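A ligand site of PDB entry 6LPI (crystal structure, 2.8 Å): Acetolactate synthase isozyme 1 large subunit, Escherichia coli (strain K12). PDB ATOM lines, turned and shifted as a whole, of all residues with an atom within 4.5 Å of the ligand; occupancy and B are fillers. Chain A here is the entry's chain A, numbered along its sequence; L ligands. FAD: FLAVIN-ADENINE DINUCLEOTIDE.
NE of Arg 285 lies within salt-bridge range of O2A of the ligand, 3.2 Å away.
The backbone carbonyl oxygen (O) of Arg 289 lies within hydrogen-bond range of a nitrogen (N3) of the ligand (3.3 Å).
O2P of the ligand sits at hydrogen-bond distance from OG1 of Thr 243, 3.1 Å away.
The backbone carbonyl oxygen (O) of Gly 414 lies within hydrogen-bond range of an oxygen (O2') of the ligand, 2.8 Å away.
The backbone NH (N) of Met 263 sits at hydrogen-bond distance from an oxygen (O4) of the ligand, at 2.9 Å.
O2 of the ligand sits at hydrogen-bond distance from N of Leu 244 (3.5 Å).
The backbone NH (N) of Ile 308 is in hydrogen-bond range of a nitrogen (N3A) of the ligand.
The backbone NH (N) of Gly 415 is in hydrogen-bond range of an oxygen (O3') of the ligand (3.3 Å).
O4 of the ligand is in hydrogen-bond range of N of His 264 (2.9 Å).
OD1 of Asp 326 lies within hydrogen-bond range of N6A of the ligand (3.0 Å).
The backbone NH (N) of Gly 220 lies within hydrogen-bond range of an oxygen (O2P) of the ligand (2.7 Å).
A nitrogen (N1A) of the ligand lies close to the backbone NH (N) of Val 327 (3.1 Å).
N3 of the ligand lies within hydrogen-bond range of O of Leu 261 (2.9 Å).
The backbone NH (N) of Arg 285 sits at hydrogen-bond distance from an oxygen (O1P) of the ligand (2.9 Å).
OD2 of Asp 307 sits at hydrogen-bond distance from O2B of the ligand, 2.5 Å away.
NH1 of Arg 162 lies within salt-bridge range of OD2 of Asp 309 (3.1 Å).
The backbone NH (N) of Asp 309 lies within hydrogen-bond range of the side-chain carboxylate (OD2) of Asp 307, at 3.1 Å.
The backbone carbonyl oxygen (O) of Ala 325 lies within hydrogen-bond range of the backbone NH (N) of Ile 308 (3.3 Å).
The backbone NH (N) of Met 263 lies within hydrogen-bond range of the backbone carbonyl oxygen (O) of Arg 289 (2.8 Å).
The backbone carbonyl oxygen (O) of Asp 307 sits at hydrogen-bond distance from the backbone NH (N) of Ala 325 (3.1 Å).
The side-chain hydroxyl (OG1) of Thr 243 sits close to the backbone NH (N) of Met 245 (3.3 Å).
The backbone NH (N) of Arg 289 lies within hydrogen-bond range of the side-chain carboxylate (OD2) of Asp 287 (2.9 Å).
The backbone NH (N) of Gly 417 lies within hydrogen-bond range of the side-chain hydroxyl (OG) of Ser 413 (3.3 Å).
The backbone carbonyl oxygen of Gly 221 sits close to a nitrogen (N7A) of the ligand (3.4 Å).
The backbone carbonyl oxygen (O) of Gly 283 sits close to an oxygen (O4B) of the ligand, 3.0 Å away.
O of Ala 325 sits close to N1A of the ligand, at 3.3 Å.
Merely in contact with the ligand: Ala 290, Met 245, Gly 219, Ala 284, Met 396, Glu 312, Arg 162, Gly 262, Asp 309, Asp 287, Met 260, Gly 265, Leu 100, Gly 417 and Val 306.
Within 4 Å of the ligand: Leu 100, Arg 162, Gly 219, Gly 220, Gly 221, Thr 243, Leu 244, Met 245, Met 260, Leu 261, Gly 262, Met 263, His 264, Gly 265, Gly 283, Ala 284, Arg 285, Asp 287, Arg 289, Ala 290, Val 306, Asp 307, Ile 308, Asp 309, Glu 312, Ala 325, Asp 326, Val 327, Met 396, Gly 414, Gly 415 and Gly 417.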
ATOM      1  N   LEU A 100      12.290  26.214 -12.043  1.00  0.00           N
ATOM      2  CA  LEU A 100      11.953  24.805 -12.211  1.00  0.00           C
ATOM      3  C   LEU A 100      10.450  24.526 -12.209  1.00  0.00           C
ATOM      4  O   LEU A 100      10.035  23.488 -12.743  1.00  0.00           O
ATOM      5  CB  LEU A 100      12.596  23.948 -11.118  1.00  0.00           C
ATOM      6  CG  LEU A 100      14.061  24.069 -10.726  1.00  0.00           C
ATOM      7  CD1 LEU A 100      14.384  22.965  -9.721  1.00  0.00           C
ATOM      8  CD2 LEU A 100      14.995  24.036 -11.867  1.00  0.00           C
ATOM      9  N   ASP A 101       9.628  25.441 -11.686  1.00  0.00           N
ATOM     10  CA  ASP A 101       8.179  25.239 -11.702  1.00  0.00           C
ATOM     11  C   ASP A 101       7.502  25.988 -12.839  1.00  0.00           C
ATOM     12  O   ASP A 101       6.285  25.843 -13.021  1.00  0.00           O
ATOM     13  CB  ASP A 101       7.562  25.660 -10.366  1.00  0.00           C
ATOM     14  CG  ASP A 101       7.758  24.614  -9.266  1.00  0.00           C
ATOM     15  OD1 ASP A 101       8.128  24.978  -8.111  1.00  0.00           O
ATOM     16  OD2 ASP A 101       7.618  23.413  -9.574  1.00  0.00           O
ATOM     17  N   SER A 102       8.283  26.718 -13.657  1.00  0.00           N
ATOM     18  CA  SER A 102       7.835  27.391 -14.871  1.00  0.00           C
ATOM     19  C   SER A 102       6.831  28.516 -14.633  1.00  0.00           C
ATOM     20  O   SER A 102       5.710  28.461 -15.136  1.00  0.00           O
ATOM     21  CB  SER A 102       7.252  26.387 -15.864  1.00  0.00           C
ATOM     22  OG  SER A 102       8.157  25.307 -16.139  1.00  0.00           O
ATOM     23  N   ARG A 162       6.851  27.931 -22.736  1.00  0.00           N
ATOM     24  CA  ARG A 162       6.926  27.507 -21.357  1.00  0.00           C
ATOM     25  C   ARG A 162       7.425  28.691 -20.547  1.00  0.00           C
ATOM     26  O   ARG A 162       8.576  29.105 -20.728  1.00  0.00           O
ATOM     27  CB  ARG A 162       7.854  26.314 -21.217  1.00  0.00           C
ATOM     28  CG  ARG A 162       8.104  25.847 -19.826  1.00  0.00           C
ATOM     29  CD  ARG A 162       9.120  24.742 -19.872  1.00  0.00           C
ATOM     30  NE  ARG A 162       9.300  24.057 -18.592  1.00  0.00           N
ATOM     31  CZ  ARG A 162       9.825  22.844 -18.495  1.00  0.00           C
ATOM     32  NH1 ARG A 162      10.200  22.207 -19.591  1.00  0.00           N
ATOM     33  NH2 ARG A 162       9.982  22.277 -17.309  1.00  0.00           N
ATOM     34  N   GLY A 219      -0.316  17.439 -15.940  1.00  0.00           N
ATOM     35  CA  GLY A 219       0.746  18.160 -15.274  1.00  0.00           C
ATOM     36  C   GLY A 219       0.431  19.646 -15.183  1.00  0.00           C
ATOM     37  O   GLY A 219      -0.634  20.110 -15.597  1.00  0.00           O
ATOM     38  N   GLY A 220       1.392  20.384 -14.626  1.00  0.00           N
ATOM     39  CA  GLY A 220       1.202  21.796 -14.390  1.00  0.00           C
ATOM     40  C   GLY A 220       1.019  22.640 -15.643  1.00  0.00           C
ATOM     41  O   GLY A 220       0.749  23.834 -15.528  1.00  0.00           O
ATOM     42  N   GLY A 221       1.198  22.065 -16.807  1.00  0.00           N
ATOM     43  CA  GLY A 221       1.061  22.822 -18.041  1.00  0.00           C
ATOM     44  C   GLY A 221      -0.328  22.948 -18.602  1.00  0.00           C
ATOM     45  O   GLY A 221      -0.533  23.718 -19.541  1.00  0.00           O
ATOM     46  N   THR A 243      -0.281  15.327 -11.451  1.00  0.00           N
ATOM     47  CA  THR A 243       0.927  15.546 -10.674  1.00  0.00           C
ATOM     48  C   THR A 243       0.636  16.480  -9.517  1.00  0.00           C
ATOM     49  O   THR A 243      -0.461  17.045  -9.411  1.00  0.00           O
ATOM     50  CB  THR A 243       2.015  16.173 -11.543  1.00  0.00           C
ATOM     51  OG1 THR A 243       1.546  17.437 -11.990  1.00  0.00           O
ATOM     52  CG2 THR A 243       2.309  15.292 -12.741  1.00  0.00           C
ATOM     53  N   LEU A 244       1.630  16.681  -8.646  1.00  0.00           N
ATOM     54  CA  LEU A 244       1.486  17.667  -7.584  1.00  0.00           C
ATOM     55  C   LEU A 244       1.120  19.055  -8.119  1.00  0.00           C
ATOM     56  O   LEU A 244       0.449  19.824  -7.434  1.00  0.00           O
ATOM     57  CB  LEU A 244       2.758  17.748  -6.748  1.00  0.00           C
ATOM     58  CG  LEU A 244       2.696  18.727  -5.570  1.00  0.00           C
ATOM     59  CD1 LEU A 244       1.711  18.229  -4.560  1.00  0.00           C
ATOM     60  CD2 LEU A 244       4.071  18.889  -4.959  1.00  0.00           C
ATOM     61  N   MET A 245       1.581  19.394  -9.317  1.00  0.00           N
ATOM     62  CA  MET A 245       1.358  20.708  -9.923  1.00  0.00           C
ATOM     63  C   MET A 245       0.016  20.821 -10.595  1.00  0.00           C
ATOM     64  O   MET A 245      -0.298  21.904 -11.102  1.00  0.00           O
ATOM     65  CB  MET A 245       2.450  21.013 -10.962  1.00  0.00           C
ATOM     66  CG  MET A 245       3.873  20.938 -10.422  1.00  0.00           C
ATOM     67  SD  MET A 245       4.038  21.950  -8.946  1.00  0.00           S
ATOM     68  CE  MET A 245       4.243  23.541  -9.784  1.00  0.00           C
ATOM     69  N   MET A 260      -3.588  12.041  -7.227  1.00  0.00           N
ATOM     70  CA  MET A 260      -2.201  12.262  -7.582  1.00  0.00           C
ATOM     71  C   MET A 260      -1.432  10.955  -7.584  1.00  0.00           C
ATOM     72  O   MET A 260      -1.641  10.100  -6.731  1.00  0.00           O
ATOM     73  CB  MET A 260      -1.561  13.237  -6.608  1.00  0.00           C
ATOM     74  CG  MET A 260      -0.072  13.199  -6.619  1.00  0.00           C
ATOM     75  SD  MET A 260       0.642  14.485  -5.576  1.00  0.00           S
ATOM     76  CE  MET A 260       0.956  13.482  -4.143  1.00  0.00           C
ATOM     77  N   LEU A 261      -0.561  10.806  -8.578  1.00  0.00           N
ATOM     78  CA  LEU A 261       0.321   9.653  -8.731  1.00  0.00           C
ATOM     79  C   LEU A 261       1.705   9.933  -8.149  1.00  0.00           C
ATOM     80  O   LEU A 261       2.078  11.061  -7.848  1.00  0.00           O
ATOM     81  CB  LEU A 261       0.426   9.297 -10.206  1.00  0.00           C
ATOM     82  CG  LEU A 261       1.474  10.089 -10.963  1.00  0.00           C
ATOM     83  CD1 LEU A 261       1.661   9.514 -12.354  1.00  0.00           C
ATOM     84  CD2 LEU A 261       1.053  11.543 -11.041  1.00  0.00           C
ATOM     85  N   GLY A 262       2.480   8.865  -7.968  1.00  0.00           N
ATOM     86  CA  GLY A 262       3.887   9.054  -7.695  1.00  0.00           C
ATOM     87  C   GLY A 262       4.396   8.771  -6.302  1.00  0.00           C
ATOM     88  O   GLY A 262       3.853   7.922  -5.595  1.00  0.00           O
ATOM     89  N   MET A 263       5.428   9.510  -5.896  1.00  0.00           N
ATOM     90  CA  MET A 263       6.248   9.137  -4.740  1.00  0.00           C
ATOM     91  C   MET A 263       5.397   8.984  -3.499  1.00  0.00           C
ATOM     92  O   MET A 263       5.584   8.045  -2.716  1.00  0.00           O
ATOM     93  CB  MET A 263       7.319  10.206  -4.503  1.00  0.00           C
ATOM     94  CG  MET A 263       7.820  10.331  -3.074  1.00  0.00           C
ATOM     95  SD  MET A 263       9.578  10.836  -2.962  1.00  0.00           S
ATOM     96  CE  MET A 263       9.585  12.516  -3.491  1.00  0.00           C
ATOM     97  N   HIS A 264       4.498   9.932  -3.271  1.00  0.00           N
ATOM     98  CA  HIS A 264       3.540   9.884  -2.184  1.00  0.00           C
ATOM     99  C   HIS A 264       2.107   9.887  -2.705  1.00  0.00           C
ATOM    100  O   HIS A 264       1.179  10.297  -2.000  1.00  0.00           O
ATOM    101  CB  HIS A 264       3.776  11.090  -1.267  1.00  0.00           C
ATOM    102  CG  HIS A 264       5.027  10.999  -0.464  1.00  0.00           C
ATOM    103  ND1 HIS A 264       6.094  11.849  -0.659  1.00  0.00           N
ATOM    104  CD2 HIS A 264       5.362  10.202   0.589  1.00  0.00           C
ATOM    105  CE1 HIS A 264       7.051  11.565   0.207  1.00  0.00           C
ATOM    106  NE2 HIS A 264       6.637  10.570   0.976  1.00  0.00           N
ATOM    107  N   GLY A 265       1.899   9.439  -3.937  1.00  0.00           N
ATOM    108  CA  GLY A 265       0.554   9.414  -4.466  1.00  0.00           C
ATOM    109  C   GLY A 265      -0.259   8.317  -3.806  1.00  0.00           C
ATOM    110  O   GLY A 265       0.135   7.676  -2.833  1.00  0.00           O
ATOM    111  N   GLY A 283       0.970  18.337 -20.495  1.00  0.00           N
ATOM    112  CA  GLY A 283       1.555  19.275 -19.549  1.00  0.00           C
ATOM    113  C   GLY A 283       2.383  18.663 -18.440  1.00  0.00           C
ATOM    114  O   GLY A 283       2.702  19.361 -17.479  1.00  0.00           O
ATOM    115  N   ALA A 284       2.764  17.395 -18.544  1.00  0.00           N
ATOM    116  CA  ALA A 284       3.664  16.781 -17.577  1.00  0.00           C
ATOM    117  C   ALA A 284       5.022  16.516 -18.209  1.00  0.00           C
ATOM    118  O   ALA A 284       5.145  16.412 -19.438  1.00  0.00           O
ATOM    119  CB  ALA A 284       3.107  15.472 -17.033  1.00  0.00           C
ATOM    120  N   ARG A 285       6.036  16.321 -17.356  1.00  0.00           N
ATOM    121  CA  ARG A 285       7.424  16.242 -17.778  1.00  0.00           C
ATOM    122  C   ARG A 285       8.125  15.000 -17.220  1.00  0.00           C
ATOM    123  O   ARG A 285       9.358  15.004 -17.057  1.00  0.00           O
ATOM    124  CB  ARG A 285       8.172  17.525 -17.350  1.00  0.00           C
ATOM    125  CG  ARG A 285       8.413  17.642 -15.854  1.00  0.00           C
ATOM    126  CD  ARG A 285       9.217  18.895 -15.491  1.00  0.00           C
ATOM    127  NE  ARG A 285       9.186  19.200 -14.049  1.00  0.00           N
ATOM    128  CZ  ARG A 285      10.148  18.867 -13.186  1.00  0.00           C
ATOM    129  NH1 ARG A 285      11.225  18.223 -13.604  1.00  0.00           N
ATOM    130  NH2 ARG A 285      10.042  19.188 -11.911  1.00  0.00           N
ATOM    131  N   PHE A 286       7.358  13.969 -16.856  1.00  0.00           N
ATOM    132  CA  PHE A 286       7.874  12.687 -16.365  1.00  0.00           C
ATOM    133  C   PHE A 286       8.935  12.864 -15.273  1.00  0.00           C
ATOM    134  O   PHE A 286       9.970  12.199 -15.280  1.00  0.00           O
ATOM    135  CB  PHE A 286       8.435  11.831 -17.509  1.00  0.00           C
ATOM    136  CG  PHE A 286       7.419  11.495 -18.552  1.00  0.00           C
ATOM    137  CD1 PHE A 286       7.299  12.301 -19.682  1.00  0.00           C
ATOM    138  CD2 PHE A 286       6.593  10.379 -18.422  1.00  0.00           C
ATOM    139  CE1 PHE A 286       6.372  12.017 -20.680  1.00  0.00           C
ATOM    140  CE2 PHE A 286       5.663  10.078 -19.418  1.00  0.00           C
ATOM    141  CZ  PHE A 286       5.554  10.910 -20.557  1.00  0.00           C
ATOM    142  N   ASP A 287       8.699  13.779 -14.345  1.00  0.00           N
ATOM    143  CA  ASP A 287       9.630  13.907 -13.236  1.00  0.00           C
ATOM    144  C   ASP A 287       9.647  12.592 -12.459  1.00  0.00           C
ATOM    145  O   ASP A 287       8.625  11.905 -12.351  1.00  0.00           O
ATOM    146  CB  ASP A 287       9.228  15.102 -12.342  1.00  0.00           C
ATOM    147  CG  ASP A 287      10.211  15.375 -11.206  1.00  0.00           C
ATOM    148  OD1 ASP A 287      11.115  16.235 -11.385  1.00  0.00           O
ATOM    149  OD2 ASP A 287      10.072  14.755 -10.131  1.00  0.00           O
ATOM    150  N   ARG A 289       9.722  11.943  -9.431  1.00  0.00           N
ATOM    151  CA  ARG A 289       8.844  11.912  -8.272  1.00  0.00           C
ATOM    152  C   ARG A 289       7.395  11.609  -8.636  1.00  0.00           C
ATOM    153  O   ARG A 289       6.634  11.159  -7.785  1.00  0.00           O
ATOM    154  CB  ARG A 289       8.935  13.242  -7.541  1.00  0.00           C
ATOM    155  CG  ARG A 289      10.171  13.366  -6.658  1.00  0.00           C
ATOM    156  CD  ARG A 289      10.387  14.785  -6.114  1.00  0.00           C
ATOM    157  NE  ARG A 289      11.251  14.789  -4.920  1.00  0.00           N
ATOM    158  CZ  ARG A 289      11.994  15.826  -4.520  1.00  0.00           C
ATOM    159  NH1 ARG A 289      12.005  16.974  -5.206  1.00  0.00           N
ATOM    160  NH2 ARG A 289      12.740  15.709  -3.428  1.00  0.00           N
ATOM    161  N   ALA A 290       7.027  11.718  -9.904  1.00  0.00           N
ATOM    162  CA  ALA A 290       5.721  11.259 -10.337  1.00  0.00           C
ATOM    163  C   ALA A 290       5.795   9.906 -11.011  1.00  0.00           C
ATOM    164  O   ALA A 290       4.811   9.157 -10.960  1.00  0.00           O
ATOM    165  CB  ALA A 290       5.077  12.252 -11.313  1.00  0.00           C
ATOM    166  N   VAL A 306       1.970  15.721 -25.223  1.00  0.00           N
ATOM    167  CA  VAL A 306       1.749  17.064 -25.758  1.00  0.00           C
ATOM    168  C   VAL A 306       2.381  18.059 -24.807  1.00  0.00           C
ATOM    169  O   VAL A 306       1.931  18.195 -23.665  1.00  0.00           O
ATOM    170  CB  VAL A 306       0.261  17.408 -25.948  1.00  0.00           C
ATOM    171  CG1 VAL A 306       0.128  18.719 -26.720  1.00  0.00           C
ATOM    172  CG2 VAL A 306      -0.446  16.317 -26.707  1.00  0.00           C
ATOM    173  N   ASP A 307       3.362  18.818 -25.305  1.00  0.00           N
ATOM    174  CA  ASP A 307       4.108  19.722 -24.455  1.00  0.00           C
ATOM    175  C   ASP A 307       4.568  20.913 -25.293  1.00  0.00           C
ATOM    176  O   ASP A 307       4.936  20.750 -26.467  1.00  0.00           O
ATOM    177  CB  ASP A 307       5.300  18.974 -23.837  1.00  0.00           C
ATOM    178  CG  ASP A 307       5.772  19.601 -22.561  1.00  0.00           C
ATOM    179  OD1 ASP A 307       5.518  18.998 -21.493  1.00  0.00           O
ATOM    180  OD2 ASP A 307       6.380  20.701 -22.629  1.00  0.00           O
ATOM    181  N   ILE A 308       4.562  22.097 -24.690  1.00  0.00           N
ATOM    182  CA  ILE A 308       4.872  23.307 -25.441  1.00  0.00           C
ATOM    183  C   ILE A 308       6.364  23.436 -25.669  1.00  0.00           C
ATOM    184  O   ILE A 308       6.784  24.206 -26.557  1.00  0.00           O
ATOM    185  CB  ILE A 308       4.354  24.571 -24.718  1.00  0.00           C
ATOM    186  CG1 ILE A 308       4.359  25.803 -25.630  1.00  0.00           C
ATOM    187  CG2 ILE A 308       5.207  24.838 -23.475  1.00  0.00           C
ATOM    188  CD1 ILE A 308       3.052  26.133 -26.281  1.00  0.00           C
ATOM    189  N   ASP A 309       7.165  22.689 -24.902  1.00  0.00           N
ATOM    190  CA  ASP A 309       8.620  22.702 -24.996  1.00  0.00           C
ATOM    191  C   ASP A 309       9.121  21.468 -25.770  1.00  0.00           C
ATOM    192  O   ASP A 309       8.960  20.328 -25.309  1.00  0.00           O
ATOM    193  CB  ASP A 309       9.206  22.788 -23.583  1.00  0.00           C
ATOM    194  CG  ASP A 309      10.728  22.739 -23.556  1.00  0.00           C
ATOM    195  OD1 ASP A 309      11.375  22.743 -24.625  1.00  0.00           O
ATOM    196  OD2 ASP A 309      11.282  22.739 -22.435  1.00  0.00           O
ATOM    197  N   GLU A 312      11.205  18.822 -23.967  1.00  0.00           N
ATOM    198  CA  GLU A 312      10.631  17.809 -23.084  1.00  0.00           C
ATOM    199  C   GLU A 312      10.212  16.559 -23.821  1.00  0.00           C
ATOM    200  O   GLU A 312      10.147  15.492 -23.202  1.00  0.00           O
ATOM    201  CB  GLU A 312       9.417  18.371 -22.339  1.00  0.00           C
ATOM    202  CG  GLU A 312       9.759  19.353 -21.230  1.00  0.00           C
ATOM    203  CD  GLU A 312      10.571  18.680 -20.152  1.00  0.00           C
ATOM    204  OE1 GLU A 312      11.450  19.345 -19.572  1.00  0.00           O
ATOM    205  OE2 GLU A 312      10.340  17.469 -19.916  1.00  0.00           O
ATOM    206  N   ALA A 325       3.020  21.724 -28.721  1.00  0.00           N
ATOM    207  CA  ALA A 325       1.960  22.691 -28.892  1.00  0.00           C
ATOM    208  C   ALA A 325       1.409  23.093 -27.536  1.00  0.00           C
ATOM    209  O   ALA A 325       1.784  22.540 -26.503  1.00  0.00           O
ATOM    210  CB  ALA A 325       0.841  22.109 -29.753  1.00  0.00           C
ATOM    211  N   ASP A 326       0.552  24.096 -27.564  1.00  0.00           N
ATOM    212  CA  ASP A 326      -0.267  24.433 -26.406  1.00  0.00           C
ATOM    213  C   ASP A 326      -1.403  23.434 -26.252  1.00  0.00           C
ATOM    214  O   ASP A 326      -2.070  23.078 -27.225  1.00  0.00           O
ATOM    215  CB  ASP A 326      -0.801  25.851 -26.564  1.00  0.00           C
ATOM    216  CG  ASP A 326      -1.920  26.121 -25.616  1.00  0.00           C
ATOM    217  OD1 ASP A 326      -1.650  26.617 -24.510  1.00  0.00           O
ATOM    218  OD2 ASP A 326      -3.072  25.823 -25.996  1.00  0.00           O
ATOM    219  N   VAL A 327      -1.654  22.980 -25.015  1.00  0.00           N
ATOM    220  CA  VAL A 327      -2.664  21.941 -24.799  1.00  0.00           C
ATOM    221  C   VAL A 327      -4.046  22.381 -25.262  1.00  0.00           C
ATOM    222  O   VAL A 327      -4.807  21.588 -25.826  1.00  0.00           O
ATOM    223  CB  VAL A 327      -2.736  21.506 -23.325  1.00  0.00           C
ATOM    224  CG1 VAL A 327      -3.390  20.128 -23.231  1.00  0.00           C
ATOM    225  CG2 VAL A 327      -1.379  21.462 -22.731  1.00  0.00           C
ATOM    226  N   VAL A 391       7.181  23.028   2.403  1.00  0.00           N
ATOM    227  CA  VAL A 391       7.712  21.775   1.890  1.00  0.00           C
ATOM    228  C   VAL A 391       8.011  20.815   3.040  1.00  0.00           C
ATOM    229  O   VAL A 391       8.659  21.181   4.020  1.00  0.00           O
ATOM    230  CB  VAL A 391       8.977  22.020   1.057  1.00  0.00           C
ATOM    231  CG1 VAL A 391       9.651  20.704   0.739  1.00  0.00           C
ATOM    232  CG2 VAL A 391       8.599  22.747  -0.235  1.00  0.00           C
ATOM    233  N   GLN A 395       3.093  19.245   3.694  1.00  0.00           N
ATOM    234  CA  GLN A 395       2.744  19.496   2.297  1.00  0.00           C
ATOM    235  C   GLN A 395       2.182  18.237   1.633  1.00  0.00           C
ATOM    236  O   GLN A 395       1.164  18.309   0.942  1.00  0.00           O
ATOM    237  CB  GLN A 395       3.976  20.012   1.542  1.00  0.00           C
ATOM    238  CG  GLN A 395       3.918  19.906  -0.006  1.00  0.00           C
ATOM    239  CD  GLN A 395       5.283  20.191  -0.665  1.00  0.00           C
ATOM    240  OE1 GLN A 395       6.321  19.938  -0.059  1.00  0.00           O
ATOM    241  NE2 GLN A 395       5.272  20.691  -1.907  1.00  0.00           N
ATOM    242  N   MET A 396       2.863  17.084   1.774  1.00  0.00           N
ATOM    243  CA  MET A 396       2.330  15.883   1.139  1.00  0.00           C
ATOM    244  C   MET A 396       0.990  15.493   1.753  1.00  0.00           C
ATOM    245  O   MET A 396       0.075  15.067   1.041  1.00  0.00           O
ATOM    246  CB  MET A 396       3.337  14.741   1.221  1.00  0.00           C
ATOM    247  CG  MET A 396       4.606  14.914   0.350  1.00  0.00           C
ATOM    248  SD  MET A 396       4.434  15.935  -1.173  1.00  0.00           S
ATOM    249  CE  MET A 396       3.241  15.040  -2.149  1.00  0.00           C
ATOM    250  N   SER A 413       5.500  24.687  -4.046  1.00  0.00           N
ATOM    251  CA  SER A 413       6.810  24.657  -4.698  1.00  0.00           C
ATOM    252  C   SER A 413       7.163  23.189  -4.941  1.00  0.00           C
ATOM    253  O   SER A 413       7.446  22.448  -4.002  1.00  0.00           O
ATOM    254  CB  SER A 413       7.830  25.358  -3.814  1.00  0.00           C
ATOM    255  OG  SER A 413       9.148  25.141  -4.248  1.00  0.00           O
ATOM    256  N   GLY A 414       7.128  22.767  -6.215  1.00  0.00           N
ATOM    257  CA  GLY A 414       7.347  21.364  -6.596  1.00  0.00           C
ATOM    258  C   GLY A 414       8.693  20.968  -7.206  1.00  0.00           C
ATOM    259  O   GLY A 414       9.255  19.916  -6.868  1.00  0.00           O
ATOM    260  N   GLY A 415       9.127  21.734  -8.187  1.00  0.00           N
ATOM    261  CA  GLY A 415      10.372  21.506  -8.883  1.00  0.00           C
ATOM    262  C   GLY A 415      11.555  21.667  -7.966  1.00  0.00           C
ATOM    263  O   GLY A 415      12.329  20.728  -7.751  1.00  0.00           O
ATOM    264  N   GLY A 417      11.236  22.611  -4.729  1.00  0.00           N
ATOM    265  CA  GLY A 417      10.808  22.134  -3.437  1.00  0.00           C
ATOM    266  C   GLY A 417      11.441  22.973  -2.353  1.00  0.00           C
ATOM    267  O   GLY A 417      12.150  22.448  -1.497  1.00  0.00           O
HETATM  268  PA  FAD L   1       5.681  20.996 -14.253  1.00  0.00           P
HETATM  269  O1A FAD L   1       4.661  21.594 -13.375  1.00  0.00           O
HETATM  270  O2A FAD L   1       7.069  21.592 -14.194  1.00  0.00           O
HETATM  271  O5B FAD L   1       5.012  21.140 -15.675  1.00  0.00           O
HETATM  272  C5B FAD L   1       5.584  21.953 -16.709  1.00  0.00           C
HETATM  273  C4B FAD L   1       5.463  21.197 -18.006  1.00  0.00           C
HETATM  274  O4B FAD L   1       4.268  21.606 -18.724  1.00  0.00           O
HETATM  275  C3B FAD L   1       6.620  21.403 -18.978  1.00  0.00           C
HETATM  276  O3B FAD L   1       6.874  20.164 -19.648  1.00  0.00           O
HETATM  277  C2B FAD L   1       6.084  22.521 -19.871  1.00  0.00           C
HETATM  278  O2B FAD L   1       6.711  22.623 -21.136  1.00  0.00           O
HETATM  279  C1B FAD L   1       4.638  22.039 -20.013  1.00  0.00           C
HETATM  280  N9A FAD L   1       3.688  23.053 -20.461  1.00  0.00           N
HETATM  281  C8A FAD L   1       3.465  24.287 -19.908  1.00  0.00           C
HETATM  282  N7A FAD L   1       2.519  24.975 -20.517  1.00  0.00           N
HETATM  283  C5A FAD L   1       2.107  24.136 -21.535  1.00  0.00           C
HETATM  284  C6A FAD L   1       1.135  24.264 -22.551  1.00  0.00           C
HETATM  285  N6A FAD L   1       0.376  25.357 -22.708  1.00  0.00           N
HETATM  286  N1A FAD L   1       0.983  23.241 -23.422  1.00  0.00           N
HETATM  287  C2A FAD L   1       1.741  22.153 -23.273  1.00  0.00           C
HETATM  288  N3A FAD L   1       2.677  21.904 -22.353  1.00  0.00           N
HETATM  289  C4A FAD L   1       2.814  22.948 -21.516  1.00  0.00           C
HETATM  290  N1  FAD L   1       5.075  15.162  -7.839  1.00  0.00           N
HETATM  291  C2  FAD L   1       4.280  14.107  -8.177  1.00  0.00           C
HETATM  292  O2  FAD L   1       3.758  14.027  -9.285  1.00  0.00           O
HETATM  293  N3  FAD L   1       4.040  13.095  -7.258  1.00  0.00           N
HETATM  294  C4  FAD L   1       4.537  13.040  -5.970  1.00  0.00           C
HETATM  295  O4  FAD L   1       4.248  12.095  -5.251  1.00  0.00           O
HETATM  296  C4X FAD L   1       5.387  14.164  -5.633  1.00  0.00           C
HETATM  297  N5  FAD L   1       5.910  14.200  -4.424  1.00  0.00           N
HETATM  298  C5X FAD L   1       6.710  15.289  -4.090  1.00  0.00           C
HETATM  299  C6  FAD L   1       7.279  15.363  -2.818  1.00  0.00           C
HETATM  300  C7  FAD L   1       8.075  16.441  -2.446  1.00  0.00           C
HETATM  301  C7M FAD L   1       8.676  16.473  -1.061  1.00  0.00           C
HETATM  302  C8  FAD L   1       8.327  17.474  -3.365  1.00  0.00           C
HETATM  303  C8M FAD L   1       9.204  18.640  -2.997  1.00  0.00           C
HETATM  304  C9  FAD L   1       7.772  17.398  -4.639  1.00  0.00           C
HETATM  305  C9A FAD L   1       6.975  16.320  -5.012  1.00  0.00           C
HETATM  306  N10 FAD L   1       6.394  16.234  -6.301  1.00  0.00           N
HETATM  307  C10 FAD L   1       5.600  15.174  -6.631  1.00  0.00           C
HETATM  308  C1' FAD L   1       6.628  17.271  -7.297  1.00  0.00           C
HETATM  309  C2' FAD L   1       7.716  16.910  -8.291  1.00  0.00           C
HETATM  310  O2' FAD L   1       8.997  17.223  -7.753  1.00  0.00           O
HETATM  311  C3' FAD L   1       7.527  17.715  -9.576  1.00  0.00           C
HETATM  312  O3' FAD L   1       7.511  19.104  -9.272  1.00  0.00           O
HETATM  313  C4' FAD L   1       6.251  17.385 -10.340  1.00  0.00           C
HETATM  314  O4' FAD L   1       6.014  15.982 -10.250  1.00  0.00           O
HETATM  315  C5' FAD L   1       6.341  17.783 -11.800  1.00  0.00           C
HETATM  316  O5' FAD L   1       5.006  17.868 -12.340  1.00  0.00           O
HETATM  317  P   FAD L   1       4.779  18.327 -13.805  1.00  0.00           P
HETATM  318  O1P FAD L   1       5.161  17.186 -14.749  1.00  0.00           O
HETATM  319  O2P FAD L   1       3.542  18.858 -13.913  1.00  0.00           O
HETATM  320  O3P FAD L   1       5.852  19.450 -13.947  1.00  0.00           O
